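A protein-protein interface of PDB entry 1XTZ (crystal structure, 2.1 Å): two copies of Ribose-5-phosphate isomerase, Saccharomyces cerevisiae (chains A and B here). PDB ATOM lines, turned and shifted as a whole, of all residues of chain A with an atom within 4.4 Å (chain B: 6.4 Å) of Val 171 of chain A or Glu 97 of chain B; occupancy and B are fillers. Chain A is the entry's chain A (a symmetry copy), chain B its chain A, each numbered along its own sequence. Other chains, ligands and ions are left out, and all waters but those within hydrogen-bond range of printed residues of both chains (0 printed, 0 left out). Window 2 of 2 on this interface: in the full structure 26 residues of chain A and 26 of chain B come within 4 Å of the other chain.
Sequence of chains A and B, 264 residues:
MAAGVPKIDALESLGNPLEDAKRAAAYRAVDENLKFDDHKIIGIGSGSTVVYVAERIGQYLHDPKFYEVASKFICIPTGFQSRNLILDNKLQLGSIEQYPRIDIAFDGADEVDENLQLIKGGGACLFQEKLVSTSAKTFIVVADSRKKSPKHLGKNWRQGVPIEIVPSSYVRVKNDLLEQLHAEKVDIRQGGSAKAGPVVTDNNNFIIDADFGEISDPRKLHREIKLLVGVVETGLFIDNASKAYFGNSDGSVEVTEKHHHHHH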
ATOM      1  N   SER A 168      15.500   5.979 -10.242  1.00  0.00           N
ATOM      2  CA  SER A 168      14.248   5.335 -10.681  1.00  0.00           C
ATOM      3  C   SER A 168      13.877   4.095  -9.866  1.00  0.00           C
ATOM      4  O   SER A 168      12.754   3.557 -10.005  1.00  0.00           O
ATOM      5  CB  SER A 168      14.387   4.988 -12.177  1.00  0.00           C
ATOM      6  OG  SER A 168      15.532   4.159 -12.334  1.00  0.00           O
ATOM      7  N   SER A 169      14.818   3.602  -9.031  1.00  0.00           N
ATOM      8  CA  SER A 169      14.624   2.358  -8.320  1.00  0.00           C
ATOM      9  C   SER A 169      14.140   2.508  -6.873  1.00  0.00           C
ATOM     10  O   SER A 169      14.084   1.525  -6.154  1.00  0.00           O
ATOM     11  CB  SER A 169      15.934   1.551  -8.305  1.00  0.00           C
ATOM     12  OG  SER A 169      16.851   2.114  -7.353  1.00  0.00           O
ATOM     13  N   TYR A 170      13.796   3.720  -6.423  1.00  0.00           N
ATOM     14  CA  TYR A 170      13.608   3.880  -4.994  1.00  0.00           C
ATOM     15  C   TYR A 170      12.425   3.068  -4.461  1.00  0.00           C
ATOM     16  O   TYR A 170      12.500   2.574  -3.352  1.00  0.00           O
ATOM     17  CB  TYR A 170      13.515   5.355  -4.575  1.00  0.00           C
ATOM     18  CG  TYR A 170      12.251   6.064  -4.995  1.00  0.00           C
ATOM     19  CD1 TYR A 170      11.108   6.087  -4.152  1.00  0.00           C
ATOM     20  CD2 TYR A 170      12.191   6.723  -6.226  1.00  0.00           C
ATOM     21  CE1 TYR A 170       9.949   6.773  -4.535  1.00  0.00           C
ATOM     22  CE2 TYR A 170      11.054   7.401  -6.604  1.00  0.00           C
ATOM     23  CZ  TYR A 170       9.937   7.412  -5.755  1.00  0.00           C
ATOM     24  OH  TYR A 170       8.826   8.101  -6.177  1.00  0.00           O
ATOM     25  N   VAL A 171      11.370   2.891  -5.264  1.00  0.00           N
ATOM     26  CA  VAL A 171      10.227   2.031  -4.825  1.00  0.00           C
ATOM     27  C   VAL A 171      10.623   0.574  -4.741  1.00  0.00           C
ATOM     28  O   VAL A 171      10.384  -0.104  -3.728  1.00  0.00           O
ATOM     29  CB  VAL A 171       8.973   2.210  -5.758  1.00  0.00           C
ATOM     30  CG1 VAL A 171       7.774   1.298  -5.261  1.00  0.00           C
ATOM     31  CG2 VAL A 171       8.542   3.722  -5.806  1.00  0.00           C
ATOM     32  N   ARG A 172      11.258   0.080  -5.808  1.00  0.00           N
ATOM     33  CA  ARG A 172      11.733  -1.297  -5.885  1.00  0.00           C
ATOM     34  C   ARG A 172      12.692  -1.596  -4.718  1.00  0.00           C
ATOM     35  O   ARG A 172      12.534  -2.591  -4.004  1.00  0.00           O
ATOM     36  CB  ARG A 172      12.447  -1.526  -7.253  1.00  0.00           C
ATOM     37  CG  ARG A 172      13.265  -2.843  -7.326  1.00  0.00           C
ATOM     38  CD  ARG A 172      12.366  -4.108  -7.167  1.00  0.00           C
ATOM     39  NE  ARG A 172      13.242  -5.262  -7.297  1.00  0.00           N
ATOM     40  CZ  ARG A 172      13.579  -5.799  -8.443  1.00  0.00           C
ATOM     41  NH1 ARG A 172      14.464  -6.797  -8.467  1.00  0.00           N
ATOM     42  NH2 ARG A 172      12.999  -5.360  -9.563  1.00  0.00           N
ATOM     43  N   VAL A 173      13.666  -0.699  -4.489  1.00  0.00           N
ATOM     44  CA  VAL A 173      14.700  -0.991  -3.497  1.00  0.00           C
ATOM     45  C   VAL A 173      14.062  -1.014  -2.098  1.00  0.00           C
ATOM     46  O   VAL A 173      14.358  -1.907  -1.270  1.00  0.00           O
ATOM     47  CB  VAL A 173      15.934   0.016  -3.548  1.00  0.00           C
ATOM     48  CG1 VAL A 173      16.922  -0.281  -2.332  1.00  0.00           C
ATOM     49  CG2 VAL A 173      16.729  -0.147  -4.861  1.00  0.00           C
ATOM     50  N   LYS A 174      13.202  -0.036  -1.831  1.00  0.00           N
ATOM     51  CA  LYS A 174      12.473  -0.020  -0.573  1.00  0.00           C
ATOM     52  C   LYS A 174      11.662  -1.315  -0.387  1.00  0.00           C
ATOM     53  O   LYS A 174      11.712  -1.931   0.695  1.00  0.00           O
ATOM     54  CB  LYS A 174      11.571   1.243  -0.491  1.00  0.00           C
ATOM     55  CG  LYS A 174      10.631   1.209   0.733  1.00  0.00           C
ATOM     56  CD  LYS A 174       9.971   2.555   1.058  1.00  0.00           C
ATOM     57  CE  LYS A 174       9.001   2.388   2.230  1.00  0.00           C
ATOM     58  NZ  LYS A 174       8.926   3.644   2.994  1.00  0.00           N
ATOM     59  N   ASN A 175      10.934  -1.731  -1.443  1.00  0.00           N
ATOM     60  CA  ASN A 175      10.197  -2.985  -1.393  1.00  0.00           C
ATOM     61  C   ASN A 175      11.081  -4.171  -1.081  1.00  0.00           C
ATOM     62  O   ASN A 175      10.714  -4.990  -0.204  1.00  0.00           O
ATOM     63  CB  ASN A 175       9.383  -3.247  -2.685  1.00  0.00           C
ATOM     64  CG  ASN A 175       8.142  -2.297  -2.830  1.00  0.00           C
ATOM     65  OD1 ASN A 175       7.645  -1.730  -1.841  1.00  0.00           O
ATOM     66  ND2 ASN A 175       7.645  -2.144  -4.083  1.00  0.00           N
ATOM     67  N   ILE B  76       5.044   0.426 -19.221  1.00  0.00           N
ATOM     68  CA  ILE B  76       6.149   0.923 -18.380  1.00  0.00           C
ATOM     69  C   ILE B  76       7.375   0.890 -19.287  1.00  0.00           C
ATOM     70  O   ILE B  76       7.685  -0.144 -19.861  1.00  0.00           O
ATOM     71  CB  ILE B  76       6.364   0.039 -17.098  1.00  0.00           C
ATOM     72  CG1 ILE B  76       5.078  -0.147 -16.285  1.00  0.00           C
ATOM     73  CG2 ILE B  76       7.496   0.597 -16.188  1.00  0.00           C
ATOM     74  CD1 ILE B  76       4.360   1.219 -15.881  1.00  0.00           C
ATOM     75  N   SER B  95       4.828   5.010 -15.085  1.00  0.00           N
ATOM     76  CA  SER B  95       6.194   4.915 -14.582  1.00  0.00           C
ATOM     77  C   SER B  95       6.321   3.729 -13.635  1.00  0.00           C
ATOM     78  O   SER B  95       5.400   3.402 -12.903  1.00  0.00           O
ATOM     79  CB  SER B  95       6.620   6.206 -13.851  1.00  0.00           C
ATOM     80  OG  SER B  95       5.910   6.269 -12.642  1.00  0.00           O
ATOM     81  N   ILE B  96       7.500   3.117 -13.633  1.00  0.00           N
ATOM     82  CA  ILE B  96       7.745   2.011 -12.721  1.00  0.00           C
ATOM     83  C   ILE B  96       7.577   2.347 -11.253  1.00  0.00           C
ATOM     84  O   ILE B  96       7.252   1.477 -10.461  1.00  0.00           O
ATOM     85  CB  ILE B  96       9.067   1.276 -13.018  1.00  0.00           C
ATOM     86  CG1 ILE B  96       8.891  -0.177 -12.518  1.00  0.00           C
ATOM     87  CG2 ILE B  96      10.307   2.080 -12.489  1.00  0.00           C
ATOM     88  CD1 ILE B  96      10.000  -0.934 -12.601  1.00  0.00           C
ATOM     89  N   GLU B  97       7.763   3.622 -10.896  1.00  0.00           N
ATOM     90  CA  GLU B  97       7.650   4.060  -9.525  1.00  0.00           C
ATOM     91  C   GLU B  97       6.193   4.010  -9.075  1.00  0.00           C
ATOM     92  O   GLU B  97       5.878   3.650  -7.937  1.00  0.00           O
ATOM     93  CB  GLU B  97       8.254   5.483  -9.366  1.00  0.00           C
ATOM     94  CG  GLU B  97       9.802   5.568  -9.638  1.00  0.00           C
ATOM     95  CD  GLU B  97      10.169   6.111 -11.028  1.00  0.00           C
ATOM     96  OE1 GLU B  97      11.184   6.828 -11.145  1.00  0.00           O
ATOM     97  OE2 GLU B  97       9.448   5.866 -12.015  1.00  0.00           O
ATOM     98  N   GLN B  98       5.289   4.372  -9.990  1.00  0.00           N
ATOM     99  CA  GLN B  98       3.867   4.393  -9.687  1.00  0.00           C
ATOM    100  C   GLN B  98       3.293   2.973  -9.862  1.00  0.00           C
ATOM    101  O   GLN B  98       2.429   2.565  -9.135  1.00  0.00           O
ATOM    102  CB  GLN B  98       3.178   5.385 -10.629  1.00  0.00           C
ATOM    103  CG  GLN B  98       1.874   5.917 -10.116  1.00  0.00           C
ATOM    104  CD  GLN B  98       1.181   6.877 -11.114  1.00  0.00           C
ATOM    105  OE1 GLN B  98      -0.055   7.015 -11.107  1.00  0.00           O
ATOM    106  NE2 GLN B  98       1.970   7.507 -11.992  1.00  0.00           N
ATOM    107  N   TYR B  99       3.795   2.237 -10.853  1.00  0.00           N
ATOM    108  CA  TYR B  99       3.369   0.857 -11.120  1.00  0.00           C
ATOM    109  C   TYR B  99       4.481  -0.182 -10.892  1.00  0.00           C
ATOM    110  O   TYR B  99       4.985  -0.751 -11.852  1.00  0.00           O
ATOM    111  CB  TYR B  99       2.840   0.788 -12.569  1.00  0.00           C
ATOM    112  CG  TYR B  99       1.726   1.798 -12.775  1.00  0.00           C
ATOM    113  CD1 TYR B  99       1.981   3.043 -13.353  1.00  0.00           C
ATOM    114  CD2 TYR B  99       0.433   1.527 -12.322  1.00  0.00           C
ATOM    115  CE1 TYR B  99       0.963   3.987 -13.513  1.00  0.00           C
ATOM    116  CE2 TYR B  99      -0.613   2.460 -12.494  1.00  0.00           C
ATOM    117  CZ  TYR B  99      -0.331   3.681 -13.074  1.00  0.00           C
ATOM    118  OH  TYR B  99      -1.336   4.586 -13.218  1.00  0.00           O
ATOM    119  N   PRO B 100       4.869  -0.416  -9.621  1.00  0.00           N
ATOM    120  CA  PRO B 100       6.046  -1.271  -9.362  1.00  0.00           C
ATOM    121  C   PRO B 100       5.821  -2.767  -9.602  1.00  0.00           C
ATOM    122  O   PRO B 100       6.787  -3.528  -9.764  1.00  0.00           O
ATOM    123  CB  PRO B 100       6.315  -1.056  -7.870  1.00  0.00           C
ATOM    124  CG  PRO B 100       4.949  -0.687  -7.274  1.00  0.00           C
ATOM    125  CD  PRO B 100       4.268   0.107  -8.366  1.00  0.00           C
ATOM    126  N   ARG B 101       4.567  -3.201  -9.618  1.00  0.00           N
ATOM    127  CA  ARG B 101       4.304  -4.628  -9.863  1.00  0.00           C
ATOM    128  C   ARG B 101       3.866  -4.797 -11.297  1.00  0.00           C
ATOM    129  O   ARG B 101       2.734  -4.484 -11.637  1.00  0.00           O
ATOM    130  CB  ARG B 101       3.273  -5.194  -8.872  1.00  0.00           C
ATOM    131  CG  ARG B 101       3.871  -5.547  -7.491  1.00  0.00           C
ATOM    132  CD  ARG B 101       4.195  -4.316  -6.656  1.00  0.00           C
ATOM    133  NE  ARG B 101       4.846  -4.628  -5.369  1.00  0.00           N
ATOM    134  CZ  ARG B 101       4.583  -4.002  -4.224  1.00  0.00           C
ATOM    135  NH1 ARG B 101       3.649  -3.033  -4.181  1.00  0.00           N
ATOM    136  NH2 ARG B 101       5.229  -4.361  -3.115  1.00  0.00           N
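The guanidinium group of Arg 101 of chain B sits close to the side-chain amide nitrogen of Asn 175 of chain A (3.4 Å).
The side-chain amide nitrogen (ND2) of Asn 175 of chain A sits close to the backbone carbonyl oxygen (O) of Val 171 of chain A (3.4 Å).
Among the printed residues, merely in contact across the chains: Ser 168 of chain A with Ile 96 of chain B (3.8 Å), Ser 168 of chain A with Glu 97 of chain B (3.4 Å), Tyr 170 of chain A with Glu 97 of chain B (3.8 Å), Val 171 of chain A with Glu 97 of chain B (3.4 Å) and Val 171 of chain A with Pro 100 of chain B (3.8 Å).
Val 171 of chain A touches two residues of chain B.
Glu 97 of chain B touches three residues of chain A.
Printed residues of chain A within 4 Å of Arg 101 of chain B: Asn 175.
Of the printed residues of chain B, Asn 175 of chain A touches Arg 101 (3.4 Å).
Of the printed residues of chain B, Ser 168 of chain A touches Ile 96 (3.8 Å) and Glu 97 (3.4 Å).
Of the printed residues of chain B, Tyr 170 of chain A touches Glu 97 (3.8 Å).
The nearest printed residue of chain A that does not touch Glu 97 of chain B is Ser 169 of chain A (5.3 Å).
Hydrophobic or aromatic side chains of chain A that line the printed part of chain B: Tyr 170 and Val 171.
Among the printed residues, no Asp or Glu carboxylate lies within 4 Å of a Lys or Arg side-chain nitrogen of the other chain.
No position is printed for both chains.
Of the 6 pairs that touch across the chains among the printed residues, none has its exchanged pair printed and touching as well.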
